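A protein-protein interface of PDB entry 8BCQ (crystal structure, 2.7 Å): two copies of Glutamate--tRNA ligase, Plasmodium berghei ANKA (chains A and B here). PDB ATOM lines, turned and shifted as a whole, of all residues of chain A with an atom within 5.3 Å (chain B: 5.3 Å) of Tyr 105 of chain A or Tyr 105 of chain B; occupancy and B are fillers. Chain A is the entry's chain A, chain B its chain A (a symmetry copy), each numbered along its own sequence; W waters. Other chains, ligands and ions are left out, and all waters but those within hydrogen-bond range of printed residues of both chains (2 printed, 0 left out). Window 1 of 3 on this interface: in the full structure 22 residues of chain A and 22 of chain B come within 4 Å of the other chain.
OH of Tyr 105 of chain B sits at hydrogen-bond distance from OH of Tyr 105 of chain A (2.6 Å). OE1 of Gln 124 of chain B lies within hydrogen-bond range of ND2 of Asn 94 of chain A (2.8 Å). The side-chain amide nitrogen of Asn 94 of chain B is in hydrogen-bond range of the side-chain amide oxygen of Gln 124 of chain A (2.8 Å).
NE2 of Gln 124 of chain A lies close to ND2 of Asn 120 of chain A, at 3.4 Å. N of Tyr 105 of chain B is in hydrogen-bond range of OD2 of Asp 96 of chain B (2.7 Å). NE2 of Gln 124 of chain B sits close to ND2 of Asn 120 of chain B (3.4 Å). The side-chain carboxylate (OD2) of Asp 96 of chain A is in hydrogen-bond range of the backbone NH (N) of Tyr 105 of chain A (2.7 Å).
Among the printed residues, pairs that only touch across the chains: Phe 97 of chain A with Tyr 105 of chain B (3.6 Å), Tyr 105 of chain A with Phe 97 of chain B (3.6 Å), Gln 124 of chain A with Phe 97 of chain B (3.9 Å) and Phe 97 of chain A with Gln 124 of chain B (3.9 Å).
Tyr 105 of chain A touches two residues of chain B. Tyr 105 of chain B touches just these residues of chain A: Phe 97 and Tyr 105. Of the printed residues of chain A, Asn 94 of chain B touches Gln 124. Of the printed residues of chain A, Gln 124 of chain B touches Asn 94 (2.8 Å) and Phe 97 (3.9 Å). Printed residues of chain B within 4 Å of Phe 97 of chain A: Tyr 105 and Gln 124. Leu 103 of chain A touches none of the printed residues of chain B. Ile 93 of chain A touches none of the printed residues of chain B.
Hydrophobic or aromatic side chains of chain A that line the printed part of chain B: Phe 97 and Tyr 105. Of the 12 printed residues of chain B, 4 touch a printed residue of chain A.
Asn 94 of chain A touches Gln 124 of chain B, and with the chains exchanged Gln 124 of chain A touches Asn 94 of chain B. Phe 97 of chain A touches Tyr 105 of chain B, and with the chains exchanged Tyr 105 of chain A touches Phe 97 of chain B. Phe 97 of chain A touches Gln 124 of chain B, and with the chains exchanged Gln 124 of chain A touches Phe 97 of chain B. Tyr 105 of chain A touches its own counterpart, Tyr 105 of chain B. Positions printed for both chains: 93, 94, 96, 97, 102, 103, 104, 105, 106, 107, 120 and 124. Of the 7 pairs that touch across the chains among the printed residues, 7 have their exchanged pair printed and touching as well.
Water W1 lies within hydrogen-bond range of OH of Tyr 105 of chain A (2.8 Å), OE1 of Gln 124 of chain B (2.8 Å) and ND2 of Asn 94 of chain A (3.1 Å). Water W2 lies within hydrogen-bond range of OH of Tyr 105 of chain B (2.8 Å), OE1 of Gln 124 of chain A (2.8 Å) and ND2 of Asn 94 of chain B (3.1 Å).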
ATOM      1  N   ILE A  93      34.981  -7.105  20.950  1.00  0.00           N
ATOM      2  CA  ILE A  93      34.322  -7.091  22.251  1.00  0.00           C
ATOM      3  C   ILE A  93      33.175  -8.092  22.271  1.00  0.00           C
ATOM      4  O   ILE A  93      32.993  -8.831  23.245  1.00  0.00           O
ATOM      5  CB  ILE A  93      33.838  -5.669  22.581  1.00  0.00           C
ATOM      6  CG1 ILE A  93      35.009  -4.685  22.532  1.00  0.00           C
ATOM      7  CG2 ILE A  93      33.140  -5.643  23.933  1.00  0.00           C
ATOM      8  CD1 ILE A  93      34.603  -3.240  22.685  1.00  0.00           C
ATOM      9  N   ASN A  94      32.382  -8.126  21.196  1.00  0.00           N
ATOM     10  CA  ASN A  94      31.288  -9.086  21.109  1.00  0.00           C
ATOM     11  C   ASN A  94      31.810 -10.517  21.103  1.00  0.00           C
ATOM     12  O   ASN A  94      31.244 -11.394  21.769  1.00  0.00           O
ATOM     13  CB  ASN A  94      30.453  -8.821  19.858  1.00  0.00           C
ATOM     14  CG  ASN A  94      29.749  -7.480  19.899  1.00  0.00           C
ATOM     15  OD1 ASN A  94      30.072  -6.573  19.134  1.00  0.00           O
ATOM     16  ND2 ASN A  94      28.774  -7.350  20.791  1.00  0.00           N
ATOM     17  N   ASP A  96      34.619 -11.667  22.412  1.00  0.00           N
ATOM     18  CA  ASP A  96      35.071 -12.005  23.758  1.00  0.00           C
ATOM     19  C   ASP A  96      33.891 -12.329  24.665  1.00  0.00           C
ATOM     20  O   ASP A  96      33.960 -13.250  25.485  1.00  0.00           O
ATOM     21  CB  ASP A  96      35.897 -10.859  24.338  1.00  0.00           C
ATOM     22  CG  ASP A  96      36.495 -11.199  25.686  1.00  0.00           C
ATOM     23  OD1 ASP A  96      37.494 -11.949  25.722  1.00  0.00           O
ATOM     24  OD2 ASP A  96      35.962 -10.719  26.712  1.00  0.00           O
ATOM     25  N   PHE A  97      32.796 -11.578  24.527  1.00  0.00           N
ATOM     26  CA  PHE A  97      31.575 -11.883  25.266  1.00  0.00           C
ATOM     27  C   PHE A  97      31.030 -13.255  24.886  1.00  0.00           C
ATOM     28  O   PHE A  97      30.658 -14.051  25.754  1.00  0.00           O
ATOM     29  CB  PHE A  97      30.532 -10.798  24.993  1.00  0.00           C
ATOM     30  CG  PHE A  97      29.293 -10.918  25.826  1.00  0.00           C
ATOM     31  CD1 PHE A  97      29.272 -10.450  27.128  1.00  0.00           C
ATOM     32  CD2 PHE A  97      28.141 -11.478  25.301  1.00  0.00           C
ATOM     33  CE1 PHE A  97      28.129 -10.552  27.897  1.00  0.00           C
ATOM     34  CE2 PHE A  97      26.996 -11.579  26.064  1.00  0.00           C
ATOM     35  CZ  PHE A  97      26.991 -11.116  27.365  1.00  0.00           C
ATOM     36  N   ASN A 102      38.082 -14.123  27.956  1.00  0.00           N
ATOM     37  CA  ASN A 102      38.649 -13.498  29.153  1.00  0.00           C
ATOM     38  C   ASN A 102      39.674 -12.422  28.787  1.00  0.00           C
ATOM     39  O   ASN A 102      40.806 -12.414  29.274  1.00  0.00           O
ATOM     40  CB  ASN A 102      39.260 -14.554  30.081  1.00  0.00           C
ATOM     41  CG  ASN A 102      39.586 -14.011  31.460  1.00  0.00           C
ATOM     42  OD1 ASN A 102      38.981 -13.044  31.918  1.00  0.00           O
ATOM     43  ND2 ASN A 102      40.549 -14.635  32.129  1.00  0.00           N
ATOM     44  N   LEU A 103      39.265 -11.503  27.913  1.00  0.00           N
ATOM     45  CA  LEU A 103      40.131 -10.407  27.496  1.00  0.00           C
ATOM     46  C   LEU A 103      39.426  -9.069  27.675  1.00  0.00           C
ATOM     47  O   LEU A 103      40.077  -8.028  27.820  1.00  0.00           O
ATOM     48  CB  LEU A 103      40.566 -10.588  26.040  1.00  0.00           C
ATOM     49  CG  LEU A 103      41.422 -11.822  25.752  1.00  0.00           C
ATOM     50  CD1 LEU A 103      41.663 -11.982  24.262  1.00  0.00           C
ATOM     51  CD2 LEU A 103      42.741 -11.737  26.506  1.00  0.00           C
ATOM     52  N   TYR A 104      38.100  -9.086  27.628  1.00  0.00           N
ATOM     53  CA  TYR A 104      37.273  -7.917  27.894  1.00  0.00           C
ATOM     54  C   TYR A 104      36.240  -8.171  28.976  1.00  0.00           C
ATOM     55  O   TYR A 104      36.041  -7.321  29.849  1.00  0.00           O
ATOM     56  CB  TYR A 104      36.569  -7.473  26.603  1.00  0.00           C
ATOM     57  CG  TYR A 104      35.829  -6.154  26.680  1.00  0.00           C
ATOM     58  CD1 TYR A 104      34.546  -6.080  27.209  1.00  0.00           C
ATOM     59  CD2 TYR A 104      36.398  -4.989  26.189  1.00  0.00           C
ATOM     60  CE1 TYR A 104      33.860  -4.881  27.262  1.00  0.00           C
ATOM     61  CE2 TYR A 104      35.720  -3.784  26.239  1.00  0.00           C
ATOM     62  CZ  TYR A 104      34.452  -3.737  26.776  1.00  0.00           C
ATOM     63  OH  TYR A 104      33.779  -2.536  26.824  1.00  0.00           O
ATOM     64  N   TYR A 105      35.583  -9.325  28.943  1.00  0.00           N
ATOM     65  CA  TYR A 105      34.679  -9.756  29.999  1.00  0.00           C
ATOM     66  C   TYR A 105      35.405 -10.800  30.834  1.00  0.00           C
ATOM     67  O   TYR A 105      35.794 -11.853  30.317  1.00  0.00           O
ATOM     68  CB  TYR A 105      33.383 -10.313  29.412  1.00  0.00           C
ATOM     69  CG  TYR A 105      32.616  -9.299  28.591  1.00  0.00           C
ATOM     70  CD1 TYR A 105      31.714  -8.428  29.190  1.00  0.00           C
ATOM     71  CD2 TYR A 105      32.803  -9.203  27.219  1.00  0.00           C
ATOM     72  CE1 TYR A 105      31.019  -7.495  28.446  1.00  0.00           C
ATOM     73  CE2 TYR A 105      32.111  -8.272  26.466  1.00  0.00           C
ATOM     74  CZ  TYR A 105      31.219  -7.423  27.082  1.00  0.00           C
ATOM     75  OH  TYR A 105      30.529  -6.504  26.326  1.00  0.00           O
ATOM     76  N   PHE A 106      35.593 -10.505  32.117  1.00  0.00           N
ATOM     77  CA  PHE A 106      36.478 -11.293  32.968  1.00  0.00           C
ATOM     78  C   PHE A 106      35.738 -12.523  33.479  1.00  0.00           C
ATOM     79  O   PHE A 106      34.820 -12.412  34.298  1.00  0.00           O
ATOM     80  CB  PHE A 106      36.998 -10.439  34.121  1.00  0.00           C
ATOM     81  CG  PHE A 106      37.885  -9.306  33.683  1.00  0.00           C
ATOM     82  CD1 PHE A 106      38.532  -9.349  32.458  1.00  0.00           C
ATOM     83  CD2 PHE A 106      38.074  -8.201  34.497  1.00  0.00           C
ATOM     84  CE1 PHE A 106      39.348  -8.309  32.052  1.00  0.00           C
ATOM     85  CE2 PHE A 106      38.890  -7.159  34.099  1.00  0.00           C
ATOM     86  CZ  PHE A 106      39.527  -7.213  32.872  1.00  0.00           C
ATOM     87  N   THR A 107      36.142 -13.695  32.996  1.00  0.00           N
ATOM     88  CA  THR A 107      35.582 -14.965  33.437  1.00  0.00           C
ATOM     89  C   THR A 107      36.325 -15.551  34.632  1.00  0.00           C
ATOM     90  O   THR A 107      35.902 -16.584  35.159  1.00  0.00           O
ATOM     91  CB  THR A 107      35.583 -15.974  32.283  1.00  0.00           C
ATOM     92  OG1 THR A 107      36.931 -16.226  31.862  1.00  0.00           O
ATOM     93  CG2 THR A 107      34.789 -15.434  31.107  1.00  0.00           C
ATOM     94  N   ASN A 120      36.212  -4.919  36.520  1.00  0.00           N
ATOM     95  CA  ASN A 120      35.932  -5.270  35.131  1.00  0.00           C
ATOM     96  C   ASN A 120      35.351  -4.080  34.375  1.00  0.00           C
ATOM     97  O   ASN A 120      35.788  -3.761  33.263  1.00  0.00           O
ATOM     98  CB  ASN A 120      34.969  -6.457  35.081  1.00  0.00           C
ATOM     99  CG  ASN A 120      35.026  -7.210  33.765  1.00  0.00           C
ATOM    100  OD1 ASN A 120      34.554  -8.342  33.673  1.00  0.00           O
ATOM    101  ND2 ASN A 120      35.621  -6.598  32.748  1.00  0.00           N
ATOM    102  N   GLN A 124      36.840  -1.876  31.034  1.00  0.00           N
ATOM    103  CA  GLN A 124      36.110  -1.686  29.785  1.00  0.00           C
ATOM    104  C   GLN A 124      36.130  -0.225  29.357  1.00  0.00           C
ATOM    105  O   GLN A 124      36.320   0.081  28.174  1.00  0.00           O
ATOM    106  CB  GLN A 124      34.676  -2.193  29.940  1.00  0.00           C
ATOM    107  CG  GLN A 124      34.588  -3.663  30.331  1.00  0.00           C
ATOM    108  CD  GLN A 124      33.179  -4.106  30.672  1.00  0.00           C
ATOM    109  OE1 GLN A 124      32.262  -3.291  30.760  1.00  0.00           O
ATOM    110  NE2 GLN A 124      32.999  -5.407  30.869  1.00  0.00           N
ATOM    111  N   ILE B  93      26.423   1.560  28.604  1.00  0.00           N
ATOM    112  CA  ILE B  93      26.646   0.132  28.419  1.00  0.00           C
ATOM    113  C   ILE B  93      27.302  -0.464  29.657  1.00  0.00           C
ATOM    114  O   ILE B  93      26.924  -1.547  30.119  1.00  0.00           O
ATOM    115  CB  ILE B  93      27.494  -0.110  27.158  1.00  0.00           C
ATOM    116  CG1 ILE B  93      26.820   0.518  25.937  1.00  0.00           C
ATOM    117  CG2 ILE B  93      27.742  -1.598  26.958  1.00  0.00           C
ATOM    118  CD1 ILE B  93      27.656   0.471  24.681  1.00  0.00           C
ATOM    119  N   ASN B  94      28.299   0.234  30.209  1.00  0.00           N
ATOM    120  CA  ASN B  94      28.952  -0.239  31.424  1.00  0.00           C
ATOM    121  C   ASN B  94      27.977  -0.283  32.593  1.00  0.00           C
ATOM    122  O   ASN B  94      27.978  -1.243  33.375  1.00  0.00           O
ATOM    123  CB  ASN B  94      30.145   0.655  31.762  1.00  0.00           C
ATOM    124  CG  ASN B  94      31.240   0.587  30.718  1.00  0.00           C
ATOM    125  OD1 ASN B  94      31.495   1.556  30.004  1.00  0.00           O
ATOM    126  ND2 ASN B  94      31.902  -0.561  30.628  1.00  0.00           N
ATOM    127  N   ASP B  96      24.696  -0.668  32.495  1.00  0.00           N
ATOM    128  CA  ASP B  96      23.791  -1.798  32.305  1.00  0.00           C
ATOM    129  C   ASP B  96      24.469  -3.108  32.686  1.00  0.00           C
ATOM    130  O   ASP B  96      23.845  -3.990  33.286  1.00  0.00           O
ATOM    131  CB  ASP B  96      23.303  -1.844  30.859  1.00  0.00           C
ATOM    132  CG  ASP B  96      22.269  -2.925  30.630  1.00  0.00           C
ATOM    133  OD1 ASP B  96      21.101  -2.725  31.026  1.00  0.00           O
ATOM    134  OD2 ASP B  96      22.625  -3.979  30.057  1.00  0.00           O
ATOM    135  N   PHE B  97      25.751  -3.249  32.344  1.00  0.00           N
ATOM    136  CA  PHE B  97      26.519  -4.417  32.765  1.00  0.00           C
ATOM    137  C   PHE B  97      26.620  -4.491  34.284  1.00  0.00           C
ATOM    138  O   PHE B  97      26.419  -5.554  34.881  1.00  0.00           O
ATOM    139  CB  PHE B  97      27.913  -4.361  32.139  1.00  0.00           C
ATOM    140  CG  PHE B  97      28.737  -5.591  32.369  1.00  0.00           C
ATOM    141  CD1 PHE B  97      28.556  -6.717  31.585  1.00  0.00           C
ATOM    142  CD2 PHE B  97      29.709  -5.614  33.354  1.00  0.00           C
ATOM    143  CE1 PHE B  97      29.318  -7.850  31.790  1.00  0.00           C
ATOM    144  CE2 PHE B  97      30.476  -6.742  33.560  1.00  0.00           C
ATOM    145  CZ  PHE B  97      30.279  -7.863  32.777  1.00  0.00           C
ATOM    146  N   ASN B 102      19.167  -4.925  32.241  1.00  0.00           N
ATOM    147  CA  ASN B 102      18.548  -5.718  31.175  1.00  0.00           C
ATOM    148  C   ASN B 102      18.125  -4.836  29.999  1.00  0.00           C
ATOM    149  O   ASN B 102      16.984  -4.877  29.537  1.00  0.00           O
ATOM    150  CB  ASN B 102      17.363  -6.526  31.717  1.00  0.00           C
ATOM    151  CG  ASN B 102      16.878  -7.587  30.745  1.00  0.00           C
ATOM    152  OD1 ASN B 102      17.634  -8.064  29.901  1.00  0.00           O
ATOM    153  ND2 ASN B 102      15.608  -7.960  30.862  1.00  0.00           N
ATOM    154  N   LEU B 103      19.066  -4.027  29.511  1.00  0.00           N
ATOM    155  CA  LEU B 103      18.807  -3.152  28.375  1.00  0.00           C
ATOM    156  C   LEU B 103      19.863  -3.348  27.295  1.00  0.00           C
ATOM    157  O   LEU B 103      19.617  -3.076  26.115  1.00  0.00           O
ATOM    158  CB  LEU B 103      18.767  -1.689  28.820  1.00  0.00           C
ATOM    159  CG  LEU B 103      17.644  -1.322  29.791  1.00  0.00           C
ATOM    160  CD1 LEU B 103      17.793   0.107  30.281  1.00  0.00           C
ATOM    161  CD2 LEU B 103      16.289  -1.527  29.133  1.00  0.00           C
ATOM    162  N   TYR B 104      21.050  -3.783  27.699  1.00  0.00           N
ATOM    163  CA  TYR B 104      22.130  -4.131  26.785  1.00  0.00           C
ATOM    164  C   TYR B 104      22.652  -5.538  27.012  1.00  0.00           C
ATOM    165  O   TYR B 104      22.887  -6.270  26.047  1.00  0.00           O
ATOM    166  CB  TYR B 104      23.281  -3.124  26.933  1.00  0.00           C
ATOM    167  CG  TYR B 104      24.390  -3.242  25.909  1.00  0.00           C
ATOM    168  CD1 TYR B 104      25.408  -4.175  26.057  1.00  0.00           C
ATOM    169  CD2 TYR B 104      24.440  -2.393  24.814  1.00  0.00           C
ATOM    170  CE1 TYR B 104      26.434  -4.271  25.136  1.00  0.00           C
ATOM    171  CE2 TYR B 104      25.462  -2.483  23.885  1.00  0.00           C
ATOM    172  CZ  TYR B 104      26.456  -3.423  24.052  1.00  0.00           C
ATOM    173  OH  TYR B 104      27.471  -3.509  23.125  1.00  0.00           O
ATOM    174  N   TYR B 105      22.831  -5.933  28.267  1.00  0.00           N
ATOM    175  CA  TYR B 105      23.183  -7.299  28.627  1.00  0.00           C
ATOM    176  C   TYR B 105      21.926  -7.979  29.150  1.00  0.00           C
ATOM    177  O   TYR B 105      21.349  -7.540  30.151  1.00  0.00           O
ATOM    178  CB  TYR B 105      24.302  -7.318  29.668  1.00  0.00           C
ATOM    179  CG  TYR B 105      25.580  -6.671  29.179  1.00  0.00           C
ATOM    180  CD1 TYR B 105      26.525  -7.400  28.468  1.00  0.00           C
ATOM    181  CD2 TYR B 105      25.836  -5.327  29.416  1.00  0.00           C
ATOM    182  CE1 TYR B 105      27.689  -6.811  28.013  1.00  0.00           C
ATOM    183  CE2 TYR B 105      26.998  -4.729  28.965  1.00  0.00           C
ATOM    184  CZ  TYR B 105      27.923  -5.474  28.268  1.00  0.00           C
ATOM    185  OH  TYR B 105      29.080  -4.875  27.826  1.00  0.00           O
ATOM    186  N   PHE B 106      21.503  -9.041  28.472  1.00  0.00           N
ATOM    187  CA  PHE B 106      20.192  -9.637  28.711  1.00  0.00           C
ATOM    188  C   PHE B 106      20.265 -10.574  29.909  1.00  0.00           C
ATOM    189  O   PHE B 106      20.889 -11.638  29.841  1.00  0.00           O
ATOM    190  CB  PHE B 106      19.709 -10.368  27.461  1.00  0.00           C
ATOM    191  CG  PHE B 106      19.451  -9.459  26.291  1.00  0.00           C
ATOM    192  CD1 PHE B 106      19.206  -8.110  26.485  1.00  0.00           C
ATOM    193  CD2 PHE B 106      19.448  -9.957  24.997  1.00  0.00           C
ATOM    194  CE1 PHE B 106      18.969  -7.271  25.412  1.00  0.00           C
ATOM    195  CE2 PHE B 106      19.210  -9.125  23.920  1.00  0.00           C
ATOM    196  CZ  PHE B 106      18.970  -7.779  24.127  1.00  0.00           C
ATOM    197  N   THR B 107      19.622 -10.180  31.006  1.00  0.00           N
ATOM    198  CA  THR B 107      19.539 -10.997  32.207  1.00  0.00           C
ATOM    199  C   THR B 107      18.330 -11.925  32.206  1.00  0.00           C
ATOM    200  O   THR B 107      18.187 -12.733  33.129  1.00  0.00           O
ATOM    201  CB  THR B 107      19.502 -10.103  33.453  1.00  0.00           C
ATOM    202  OG1 THR B 107      18.333  -9.275  33.419  1.00  0.00           O
ATOM    203  CG2 THR B 107      20.735  -9.219  33.506  1.00  0.00           C
ATOM    204  N   ASN B 120      21.711 -11.938  21.950  1.00  0.00           N
ATOM    205  CA  ASN B 120      22.227 -10.821  22.735  1.00  0.00           C
ATOM    206  C   ASN B 120      23.384 -10.138  22.015  1.00  0.00           C
ATOM    207  O   ASN B 120      23.424  -8.907  21.906  1.00  0.00           O
ATOM    208  CB  ASN B 120      22.671 -11.318  24.111  1.00  0.00           C
ATOM    209  CG  ASN B 120      22.723 -10.213  25.151  1.00  0.00           C
ATOM    210  OD1 ASN B 120      22.763 -10.485  26.349  1.00  0.00           O
ATOM    211  ND2 ASN B 120      22.701  -8.964  24.701  1.00  0.00           N
ATOM    212  N   GLN B 124      23.794  -6.169  20.492  1.00  0.00           N
ATOM    213  CA  GLN B 124      24.866  -5.253  20.868  1.00  0.00           C
ATOM    214  C   GLN B 124      25.492  -4.611  19.639  1.00  0.00           C
ATOM    215  O   GLN B 124      25.768  -3.405  19.630  1.00  0.00           O
ATOM    216  CB  GLN B 124      25.915  -5.993  21.696  1.00  0.00           C
ATOM    217  CG  GLN B 124      25.356  -6.628  22.964  1.00  0.00           C
ATOM    218  CD  GLN B 124      26.354  -7.520  23.675  1.00  0.00           C
ATOM    219  OE1 GLN B 124      27.437  -7.795  23.161  1.00  0.00           O
ATOM    220  NE2 GLN B 124      25.991  -7.981  24.866  1.00  0.00           N
HETATM  221  O   HOH W   1      30.053  -6.916  23.621  1.00  0.00           O
HETATM  222  O   HOH W   2      30.120  -2.629  29.086  1.00  0.00           O
